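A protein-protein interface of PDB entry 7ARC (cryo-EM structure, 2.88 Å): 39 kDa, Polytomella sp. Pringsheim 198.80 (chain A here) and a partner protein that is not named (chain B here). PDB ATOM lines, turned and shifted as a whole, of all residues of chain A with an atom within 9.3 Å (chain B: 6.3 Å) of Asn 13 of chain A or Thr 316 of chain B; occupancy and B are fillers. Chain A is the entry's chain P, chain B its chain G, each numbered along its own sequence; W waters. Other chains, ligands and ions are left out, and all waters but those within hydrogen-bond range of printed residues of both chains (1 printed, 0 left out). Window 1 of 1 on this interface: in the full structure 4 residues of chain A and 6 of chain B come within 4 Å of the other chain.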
ATOM      1  N   PRO A   6     -24.180  21.114  -8.848  1.00  0.00           N
ATOM      2  CA  PRO A   6     -23.166  20.057  -8.867  1.00  0.00           C
ATOM      3  C   PRO A   6     -22.473  19.913  -7.522  1.00  0.00           C
ATOM      4  O   PRO A   6     -22.384  20.857  -6.735  1.00  0.00           O
ATOM      5  CB  PRO A   6     -22.181  20.542  -9.937  1.00  0.00           C
ATOM      6  CG  PRO A   6     -22.516  22.008 -10.116  1.00  0.00           C
ATOM      7  CD  PRO A   6     -23.991  22.026  -9.981  1.00  0.00           C
ATOM      8  N   PHE A   7     -21.976  18.708  -7.268  1.00  0.00           N
ATOM      9  CA  PHE A   7     -20.993  18.490  -6.214  1.00  0.00           C
ATOM     10  C   PHE A   7     -19.672  19.122  -6.643  1.00  0.00           C
ATOM     11  O   PHE A   7     -19.060  18.680  -7.619  1.00  0.00           O
ATOM     12  CB  PHE A   7     -20.825  16.995  -5.966  1.00  0.00           C
ATOM     13  CG  PHE A   7     -21.729  16.445  -4.903  1.00  0.00           C
ATOM     14  CD1 PHE A   7     -21.679  16.917  -3.608  1.00  0.00           C
ATOM     15  CD2 PHE A   7     -22.630  15.440  -5.208  1.00  0.00           C
ATOM     16  CE1 PHE A   7     -22.518  16.404  -2.640  1.00  0.00           C
ATOM     17  CE2 PHE A   7     -23.466  14.923  -4.244  1.00  0.00           C
ATOM     18  CZ  PHE A   7     -23.409  15.405  -2.958  1.00  0.00           C
ATOM     19  N   ASP A   8     -19.223  20.159  -5.930  1.00  0.00           N
ATOM     20  CA  ASP A   8     -18.018  20.890  -6.335  1.00  0.00           C
ATOM     21  C   ASP A   8     -16.791  20.055  -5.986  1.00  0.00           C
ATOM     22  O   ASP A   8     -16.099  20.274  -4.990  1.00  0.00           O
ATOM     23  CB  ASP A   8     -17.953  22.271  -5.692  1.00  0.00           C
ATOM     24  CG  ASP A   8     -19.003  23.218  -6.233  1.00  0.00           C
ATOM     25  OD1 ASP A   8     -19.401  23.057  -7.405  1.00  0.00           O
ATOM     26  OD2 ASP A   8     -19.393  24.154  -5.508  1.00  0.00           O
ATOM     27  N   LEU A   9     -16.521  19.081  -6.848  1.00  0.00           N
ATOM     28  CA  LEU A   9     -15.338  18.242  -6.769  1.00  0.00           C
ATOM     29  C   LEU A   9     -14.620  18.309  -8.107  1.00  0.00           C
ATOM     30  O   LEU A   9     -15.256  18.445  -9.155  1.00  0.00           O
ATOM     31  CB  LEU A   9     -15.716  16.799  -6.438  1.00  0.00           C
ATOM     32  CG  LEU A   9     -16.022  16.512  -4.970  1.00  0.00           C
ATOM     33  CD1 LEU A   9     -15.973  15.031  -4.705  1.00  0.00           C
ATOM     34  CD2 LEU A   9     -15.050  17.238  -4.071  1.00  0.00           C
ATOM     35  N   ASN A  10     -13.292  18.238  -8.074  1.00  0.00           N
ATOM     36  CA  ASN A  10     -12.540  18.382  -9.311  1.00  0.00           C
ATOM     37  C   ASN A  10     -12.834  17.217 -10.247  1.00  0.00           C
ATOM     38  O   ASN A  10     -12.883  16.057  -9.827  1.00  0.00           O
ATOM     39  CB  ASN A  10     -11.042  18.459  -9.023  1.00  0.00           C
ATOM     40  CG  ASN A  10     -10.656  19.715  -8.266  1.00  0.00           C
ATOM     41  OD1 ASN A  10     -10.847  20.831  -8.752  1.00  0.00           O
ATOM     42  ND2 ASN A  10     -10.096  19.539  -7.075  1.00  0.00           N
ATOM     43  N   ALA A  11     -13.045  17.543 -11.522  1.00  0.00           N
ATOM     44  CA  ALA A  11     -13.344  16.588 -12.587  1.00  0.00           C
ATOM     45  C   ALA A  11     -14.669  15.868 -12.367  1.00  0.00           C
ATOM     46  O   ALA A  11     -14.904  14.805 -12.949  1.00  0.00           O
ATOM     47  CB  ALA A  11     -12.212  15.568 -12.762  1.00  0.00           C
ATOM     48  N   ASN A  12     -15.545  16.422 -11.526  1.00  0.00           N
ATOM     49  CA  ASN A  12     -16.875  15.846 -11.352  1.00  0.00           C
ATOM     50  C   ASN A  12     -17.691  15.934 -12.635  1.00  0.00           C
ATOM     51  O   ASN A  12     -18.413  14.996 -12.986  1.00  0.00           O
ATOM     52  CB  ASN A  12     -17.599  16.545 -10.204  1.00  0.00           C
ATOM     53  CG  ASN A  12     -18.894  15.859  -9.823  1.00  0.00           C
ATOM     54  OD1 ASN A  12     -19.290  14.862 -10.417  1.00  0.00           O
ATOM     55  ND2 ASN A  12     -19.565  16.400  -8.822  1.00  0.00           N
ATOM     56  N   ASN A  13     -17.582  17.057 -13.348  1.00  0.00           N
ATOM     57  CA  ASN A  13     -18.350  17.274 -14.571  1.00  0.00           C
ATOM     58  C   ASN A  13     -18.182  16.147 -15.584  1.00  0.00           C
ATOM     59  O   ASN A  13     -19.124  15.825 -16.316  1.00  0.00           O
ATOM     60  CB  ASN A  13     -17.984  18.630 -15.179  1.00  0.00           C
ATOM     61  CG  ASN A  13     -16.531  18.722 -15.589  1.00  0.00           C
ATOM     62  OD1 ASN A  13     -15.792  17.742 -15.540  1.00  0.00           O
ATOM     63  ND2 ASN A  13     -16.114  19.911 -16.000  1.00  0.00           N
ATOM     64  N   ALA A  14     -16.999  15.538 -15.644  1.00  0.00           N
ATOM     65  CA  ALA A  14     -16.781  14.426 -16.563  1.00  0.00           C
ATOM     66  C   ALA A  14     -17.544  13.183 -16.122  1.00  0.00           C
ATOM     67  O   ALA A  14     -18.322  12.608 -16.891  1.00  0.00           O
ATOM     68  CB  ALA A  14     -15.285  14.128 -16.672  1.00  0.00           C
ATOM     69  N   VAL A  15     -17.324  12.746 -14.881  1.00  0.00           N
ATOM     70  CA  VAL A  15     -17.874  11.473 -14.419  1.00  0.00           C
ATOM     71  C   VAL A  15     -19.388  11.545 -14.222  1.00  0.00           C
ATOM     72  O   VAL A  15     -20.103  10.588 -14.538  1.00  0.00           O
ATOM     73  CB  VAL A  15     -17.140  11.018 -13.146  1.00  0.00           C
ATOM     74  CG1 VAL A  15     -15.679  10.779 -13.453  1.00  0.00           C
ATOM     75  CG2 VAL A  15     -17.241  12.079 -12.081  1.00  0.00           C
ATOM     76  N   ARG A  16     -19.903  12.651 -13.683  1.00  0.00           N
ATOM     77  CA  ARG A  16     -21.321  12.726 -13.343  1.00  0.00           C
ATOM     78  C   ARG A  16     -22.186  12.528 -14.583  1.00  0.00           C
ATOM     79  O   ARG A  16     -21.849  12.994 -15.674  1.00  0.00           O
ATOM     80  CB  ARG A  16     -21.674  14.073 -12.713  1.00  0.00           C
ATOM     81  CG  ARG A  16     -21.514  15.227 -13.671  1.00  0.00           C
ATOM     82  CD  ARG A  16     -21.803  16.575 -13.066  1.00  0.00           C
ATOM     83  NE  ARG A  16     -21.621  17.600 -14.086  1.00  0.00           N
ATOM     84  CZ  ARG A  16     -21.812  18.896 -13.897  1.00  0.00           C
ATOM     85  NH1 ARG A  16     -22.213  19.370 -12.734  1.00  0.00           N
ATOM     86  NH2 ARG A  16     -21.607  19.736 -14.907  1.00  0.00           N
ATOM     87  N   ASN A  17     -23.297  11.812 -14.417  1.00  0.00           N
ATOM     88  CA  ASN A  17     -24.264  11.682 -15.497  1.00  0.00           C
ATOM     89  C   ASN A  17     -25.547  11.087 -14.935  1.00  0.00           C
ATOM     90  O   ASN A  17     -25.500  10.234 -14.049  1.00  0.00           O
ATOM     91  CB  ASN A  17     -23.714  10.815 -16.638  1.00  0.00           C
ATOM     92  CG  ASN A  17     -24.598  10.837 -17.868  1.00  0.00           C
ATOM     93  OD1 ASN A  17     -25.655  11.466 -17.880  1.00  0.00           O
ATOM     94  ND2 ASN A  17     -24.137  10.199 -18.934  1.00  0.00           N
ATOM     95  N   GLY A  18     -26.682  11.546 -15.455  1.00  0.00           N
ATOM     96  CA  GLY A  18     -27.976  11.117 -14.979  1.00  0.00           C
ATOM     97  C   GLY A  18     -28.712  12.219 -14.246  1.00  0.00           C
ATOM     98  O   GLY A  18     -28.174  13.304 -14.008  1.00  0.00           O
ATOM     99  N   ILE A  25     -25.240   8.566 -11.728  1.00  0.00           N
ATOM    100  CA  ILE A  25     -23.824   8.546 -11.383  1.00  0.00           C
ATOM    101  C   ILE A  25     -23.458   9.904 -10.805  1.00  0.00           C
ATOM    102  O   ILE A  25     -23.551  10.927 -11.492  1.00  0.00           O
ATOM    103  CB  ILE A  25     -22.935   8.221 -12.592  1.00  0.00           C
ATOM    104  CG1 ILE A  25     -23.363   6.917 -13.255  1.00  0.00           C
ATOM    105  CG2 ILE A  25     -21.479   8.151 -12.175  1.00  0.00           C
ATOM    106  CD1 ILE A  25     -22.626   6.644 -14.539  1.00  0.00           C
ATOM    107  N   GLY A  26     -23.045   9.913  -9.546  1.00  0.00           N
ATOM    108  CA  GLY A  26     -22.429  11.075  -8.927  1.00  0.00           C
ATOM    109  C   GLY A  26     -20.943  10.810  -8.760  1.00  0.00           C
ATOM    110  O   GLY A  26     -20.537   9.686  -8.454  1.00  0.00           O
ATOM    111  N   GLY A  27     -20.138  11.841  -8.977  1.00  0.00           N
ATOM    112  CA  GLY A  27     -18.703  11.654  -8.971  1.00  0.00           C
ATOM    113  C   GLY A  27     -18.088  11.703  -7.590  1.00  0.00           C
ATOM    114  O   GLY A  27     -16.934  12.112  -7.436  1.00  0.00           O
ATOM    115  N   VAL A  28     -18.839  11.281  -6.581  1.00  0.00           N
ATOM    116  CA  VAL A  28     -18.407  11.347  -5.192  1.00  0.00           C
ATOM    117  C   VAL A  28     -18.260   9.930  -4.663  1.00  0.00           C
ATOM    118  O   VAL A  28     -19.236   9.175  -4.610  1.00  0.00           O
ATOM    119  CB  VAL A  28     -19.395  12.152  -4.333  1.00  0.00           C
ATOM    120  CG1 VAL A  28     -19.042  12.036  -2.870  1.00  0.00           C
ATOM    121  CG2 VAL A  28     -19.405  13.605  -4.767  1.00  0.00           C
ATOM    122  N   LEU B 314     -13.454  15.556 -26.970  1.00  0.00           N
ATOM    123  CA  LEU B 314     -13.484  16.571 -25.926  1.00  0.00           C
ATOM    124  C   LEU B 314     -14.753  16.408 -25.103  1.00  0.00           C
ATOM    125  O   LEU B 314     -15.860  16.415 -25.652  1.00  0.00           O
ATOM    126  CB  LEU B 314     -13.432  17.971 -26.530  1.00  0.00           C
ATOM    127  CG  LEU B 314     -12.202  18.363 -27.340  1.00  0.00           C
ATOM    128  CD1 LEU B 314     -12.421  19.714 -27.986  1.00  0.00           C
ATOM    129  CD2 LEU B 314     -10.996  18.391 -26.447  1.00  0.00           C
ATOM    130  N   ASN B 315     -14.594  16.263 -23.791  1.00  0.00           N
ATOM    131  CA  ASN B 315     -15.714  16.023 -22.894  1.00  0.00           C
ATOM    132  C   ASN B 315     -15.964  17.150 -21.904  1.00  0.00           C
ATOM    133  O   ASN B 315     -17.105  17.329 -21.480  1.00  0.00           O
ATOM    134  CB  ASN B 315     -15.510  14.711 -22.119  1.00  0.00           C
ATOM    135  CG  ASN B 315     -14.281  14.739 -21.237  1.00  0.00           C
ATOM    136  OD1 ASN B 315     -13.303  15.417 -21.539  1.00  0.00           O
ATOM    137  ND2 ASN B 315     -14.326  13.999 -20.137  1.00  0.00           N
ATOM    138  N   THR B 316     -14.941  17.907 -21.520  1.00  0.00           N
ATOM    139  CA  THR B 316     -15.066  18.897 -20.464  1.00  0.00           C
ATOM    140  C   THR B 316     -14.430  20.207 -20.900  1.00  0.00           C
ATOM    141  O   THR B 316     -13.530  20.216 -21.746  1.00  0.00           O
ATOM    142  CB  THR B 316     -14.399  18.422 -19.164  1.00  0.00           C
ATOM    143  OG1 THR B 316     -13.036  18.064 -19.421  1.00  0.00           O
ATOM    144  CG2 THR B 316     -15.130  17.221 -18.603  1.00  0.00           C
ATOM    145  N   PRO B 317     -14.892  21.332 -20.357  1.00  0.00           N
ATOM    146  CA  PRO B 317     -14.211  22.606 -20.615  1.00  0.00           C
ATOM    147  C   PRO B 317     -12.796  22.594 -20.061  1.00  0.00           C
ATOM    148  O   PRO B 317     -12.536  22.063 -18.980  1.00  0.00           O
ATOM    149  CB  PRO B 317     -15.094  23.626 -19.891  1.00  0.00           C
ATOM    150  CG  PRO B 317     -16.430  22.976 -19.843  1.00  0.00           C
ATOM    151  CD  PRO B 317     -16.131  21.534 -19.591  1.00  0.00           C
ATOM    152  N   LEU B 318     -11.875  23.179 -20.820  1.00  0.00           N
ATOM    153  CA  LEU B 318     -10.471  23.244 -20.442  1.00  0.00           C
ATOM    154  C   LEU B 318     -10.005  24.689 -20.476  1.00  0.00           C
ATOM    155  O   LEU B 318     -10.239  25.393 -21.461  1.00  0.00           O
ATOM    156  CB  LEU B 318      -9.606  22.396 -21.376  1.00  0.00           C
ATOM    157  CG  LEU B 318      -9.953  20.917 -21.506  1.00  0.00           C
ATOM    158  CD1 LEU B 318      -9.250  20.331 -22.710  1.00  0.00           C
ATOM    159  CD2 LEU B 318      -9.570  20.167 -20.251  1.00  0.00           C
ATOM    160  N   ASN B 327      -8.801  20.754 -16.382  1.00  0.00           N
ATOM    161  CA  ASN B 327     -10.249  20.661 -16.239  1.00  0.00           C
ATOM    162  C   ASN B 327     -10.846  21.913 -15.609  1.00  0.00           C
ATOM    163  O   ASN B 327     -10.359  22.415 -14.595  1.00  0.00           O
ATOM    164  CB  ASN B 327     -10.610  19.436 -15.398  1.00  0.00           C
ATOM    165  CG  ASN B 327     -12.095  19.153 -15.391  1.00  0.00           C
ATOM    166  OD1 ASN B 327     -12.843  19.720 -14.599  1.00  0.00           O
ATOM    167  ND2 ASN B 327     -12.530  18.268 -16.277  1.00  0.00           N
ATOM    168  N   ALA B 328     -11.947  22.385 -16.184  1.00  0.00           N
ATOM    169  CA  ALA B 328     -12.640  23.544 -15.647  1.00  0.00           C
ATOM    170  C   ALA B 328     -14.134  23.374 -15.855  1.00  0.00           C
ATOM    171  O   ALA B 328     -14.580  22.621 -16.723  1.00  0.00           O
ATOM    172  CB  ALA B 328     -12.157  24.843 -16.301  1.00  0.00           C
ATOM    173  N   THR B 329     -14.904  24.075 -15.030  1.00  0.00           N
ATOM    174  CA  THR B 329     -16.349  24.097 -15.173  1.00  0.00           C
ATOM    175  C   THR B 329     -16.761  25.113 -16.234  1.00  0.00           C
ATOM    176  O   THR B 329     -15.967  25.938 -16.689  1.00  0.00           O
ATOM    177  CB  THR B 329     -17.013  24.419 -13.837  1.00  0.00           C
ATOM    178  OG1 THR B 329     -16.906  25.822 -13.576  1.00  0.00           O
ATOM    179  CG2 THR B 329     -16.339  23.652 -12.714  1.00  0.00           C
ATOM    180  N   TRP B 330     -18.031  25.040 -16.632  1.00  0.00           N
ATOM    181  CA  TRP B 330     -18.535  25.939 -17.664  1.00  0.00           C
ATOM    182  C   TRP B 330     -18.462  27.392 -17.213  1.00  0.00           C
ATOM    183  O   TRP B 330     -18.175  28.285 -18.018  1.00  0.00           O
ATOM    184  CB  TRP B 330     -19.966  25.564 -18.033  1.00  0.00           C
ATOM    185  CG  TRP B 330     -20.049  24.525 -19.100  1.00  0.00           C
ATOM    186  CD1 TRP B 330     -20.514  23.256 -18.962  1.00  0.00           C
ATOM    187  CD2 TRP B 330     -19.651  24.660 -20.467  1.00  0.00           C
ATOM    188  NE1 TRP B 330     -20.436  22.588 -20.156  1.00  0.00           N
ATOM    189  CE2 TRP B 330     -19.910  23.429 -21.099  1.00  0.00           C
ATOM    190  CE3 TRP B 330     -19.105  25.701 -21.221  1.00  0.00           C
ATOM    191  CZ2 TRP B 330     -19.641  23.212 -22.444  1.00  0.00           C
ATOM    192  CZ3 TRP B 330     -18.841  25.482 -22.555  1.00  0.00           C
ATOM    193  CH2 TRP B 330     -19.108  24.249 -23.153  1.00  0.00           C
ATOM    194  N   VAL B 587     -10.948  25.638 -24.104  1.00  0.00           N
ATOM    195  CA  VAL B 587     -11.561  24.633 -24.963  1.00  0.00           C
ATOM    196  C   VAL B 587     -12.992  24.429 -24.492  1.00  0.00           C
ATOM    197  O   VAL B 587     -13.227  24.129 -23.317  1.00  0.00           O
ATOM    198  CB  VAL B 587     -10.777  23.313 -24.934  1.00  0.00           C
ATOM    199  CG1 VAL B 587     -11.624  22.185 -25.474  1.00  0.00           C
ATOM    200  CG2 VAL B 587      -9.491  23.442 -25.722  1.00  0.00           C
ATOM    201  N   LEU B 588     -13.949  24.601 -25.400  1.00  0.00           N
ATOM    202  CA  LEU B 588     -15.356  24.417 -25.070  1.00  0.00           C
ATOM    203  C   LEU B 588     -15.893  23.182 -25.779  1.00  0.00           C
ATOM    204  O   LEU B 588     -15.982  23.179 -27.016  1.00  0.00           O
ATOM    205  CB  LEU B 588     -16.165  25.652 -25.466  1.00  0.00           C
ATOM    206  CG  LEU B 588     -15.667  26.981 -24.900  1.00  0.00           C
ATOM    207  CD1 LEU B 588     -16.427  28.133 -25.521  1.00  0.00           C
ATOM    208  CD2 LEU B 588     -15.770  27.016 -23.391  1.00  0.00           C
ATOM    209  N   PRO B 589     -16.258  22.121 -25.062  1.00  0.00           N
ATOM    210  CA  PRO B 589     -16.736  20.910 -25.737  1.00  0.00           C
ATOM    211  C   PRO B 589     -18.073  21.141 -26.422  1.00  0.00           C
ATOM    212  O   PRO B 589     -18.954  21.820 -25.893  1.00  0.00           O
ATOM    213  CB  PRO B 589     -16.861  19.894 -24.598  1.00  0.00           C
ATOM    214  CG  PRO B 589     -17.019  20.717 -23.379  1.00  0.00           C
ATOM    215  CD  PRO B 589     -16.231  21.966 -23.600  1.00  0.00           C
ATOM    216  N   LEU B 617     -21.795  13.649 -25.050  1.00  0.00           N
ATOM    217  CA  LEU B 617     -20.834  12.987 -24.182  1.00  0.00           C
ATOM    218  C   LEU B 617     -20.308  13.944 -23.124  1.00  0.00           C
ATOM    219  O   LEU B 617     -19.919  15.073 -23.438  1.00  0.00           O
ATOM    220  CB  LEU B 617     -19.663  12.452 -25.004  1.00  0.00           C
ATOM    221  CG  LEU B 617     -18.610  11.678 -24.219  1.00  0.00           C
ATOM    222  CD1 LEU B 617     -19.200  10.422 -23.597  1.00  0.00           C
ATOM    223  CD2 LEU B 617     -17.434  11.359 -25.106  1.00  0.00           C
ATOM    224  N   GLY B 618     -20.279  13.475 -21.879  1.00  0.00           N
ATOM    225  CA  GLY B 618     -19.656  14.236 -20.811  1.00  0.00           C
ATOM    226  C   GLY B 618     -20.349  15.562 -20.593  1.00  0.00           C
ATOM    227  O   GLY B 618     -21.572  15.682 -20.705  1.00  0.00           O
ATOM    228  N   ASP B 619     -19.557  16.575 -20.264  1.00  0.00           N
ATOM    229  CA  ASP B 619     -20.077  17.919 -20.025  1.00  0.00           C
ATOM    230  C   ASP B 619     -19.988  18.762 -21.296  1.00  0.00           C
ATOM    231  O   ASP B 619     -19.450  19.866 -21.304  1.00  0.00           O
ATOM    232  CB  ASP B 619     -19.315  18.559 -18.871  1.00  0.00           C
ATOM    233  CG  ASP B 619     -19.928  19.865 -18.409  1.00  0.00           C
ATOM    234  OD1 ASP B 619     -20.936  20.301 -19.001  1.00  0.00           O
ATOM    235  OD2 ASP B 619     -19.403  20.456 -17.443  1.00  0.00           O
ATOM    236  N   ALA B 620     -20.520  18.231 -22.393  1.00  0.00           N
ATOM    237  CA  ALA B 620     -20.591  18.933 -23.666  1.00  0.00           C
ATOM    238  C   ALA B 620     -22.017  19.394 -23.940  1.00  0.00           C
ATOM    239  O   ALA B 620     -22.985  18.837 -23.418  1.00  0.00           O
ATOM    240  CB  ALA B 620     -20.104  18.041 -24.810  1.00  0.00           C
HETATM  241  O   HOH W   1     -19.579  22.230 -15.646  1.00  0.00           O
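The side-chain amide nitrogen (ND2) of Asn 327 of chain B lies within hydrogen-bond range of the side-chain amide oxygen (OD1) of Asn 13 of chain A, at 3.4 Å.
O of Ala 328 of chain B is in hydrogen-bond range of ND2 of Asn 13 of chain A (3.2 Å).
The side-chain carboxylate of Asp 619 of chain B is in salt-bridge range of the guanidinium group of Arg 16 of chain A, at 3.4 Å.
The side-chain hydroxyl of Thr 316 of chain B is in hydrogen-bond range of the side-chain amide oxygen of Asn 315 of chain B (3.4 Å).
The backbone carbonyl oxygen (O) of Asn 315 of chain B sits at hydrogen-bond distance from the backbone NH (N) of Asp 619 of chain B.
OG1 of Thr 316 of chain B lies within hydrogen-bond range of ND2 of Asn 327 of chain B (3.2 Å).
The backbone NH (N) of Ala 328 of chain B is in hydrogen-bond range of the backbone carbonyl oxygen (O) of Pro 317 of chain B, 2.9 Å away.
OD1 of Asp 619 of chain B is in hydrogen-bond range of NE1 of Trp 330 of chain B (2.6 Å).
Among the printed residues, pairs that only touch across the chains: Ala 11 of chain A with Asn 327 of chain B, Asn 13 of chain A with Thr 316 of chain B, Asn 13 of chain A with Pro 317 of chain B, Asn 13 of chain A with Asp 619 of chain B, Ala 14 of chain A with Asn 315 of chain B and Ala 14 of chain A with Thr 316 of chain B.
Asn 10 of chain A touches none of the printed residues of chain B.
Of the printed residues of chain B, Ala 11 of chain A touches Asn 327 (3.8 Å).
Of the printed residues of chain B, Asn 13 of chain A touches Thr 316, Pro 317, Asn 327, Ala 328 and Asp 619.
Of the printed residues of chain B, Ala 14 of chain A touches Asn 315 (3.6 Å) and Thr 316 (3.6 Å).
Printed residues of chain B within 4 Å of Arg 16 of chain A: Asp 619.
Asn 315 of chain B touches just one residue of chain A: Ala 14.
Of chain A, only Asn 13 comes within 4 Å of Pro 317 of chain B.
Printed residues of chain A within 4 Å of Asn 327 of chain B: Ala 11 and Asn 13.
Of the printed residues of chain A, Ala 328 of chain B touches Asn 13 (3.2 Å).
Of chain A, only Asn 13 (3.2 Å) and Arg 16 (3.4 Å) come within 4 Å of Asp 619 of chain B.
Ala 620 of chain B touches none of the printed residues of chain A.
The nearest residue of chain B that does not touch Asn 13 of chain A is Thr 329 of chain B (4.3 Å).
Hydrophobic or aromatic side chains of chain A that line the printed part of chain B: Ala 14.
Along chain A the printed residues that touch a printed residue of chain B span positions 11 to 16.
Hydrophobic or aromatic side chains of chain B that line the printed part of chain A: Pro 317.
Among the printed residues, 9 pairs touch across the chains.
Among the printed residues, Asp or Glu carboxylates within 4 Å of a Lys or Arg side-chain nitrogen of the other chain: Arg 16 of chain A with Asp 619 of chain B.
Water W1 lies within hydrogen-bond range of the side-chain carboxylate of Asp 619 of chain B (2.5 Å), the guanidinium group of Arg 16 of chain A (3.3 Å) and the backbone NH of Trp 330 of chain B (3.4 Å).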
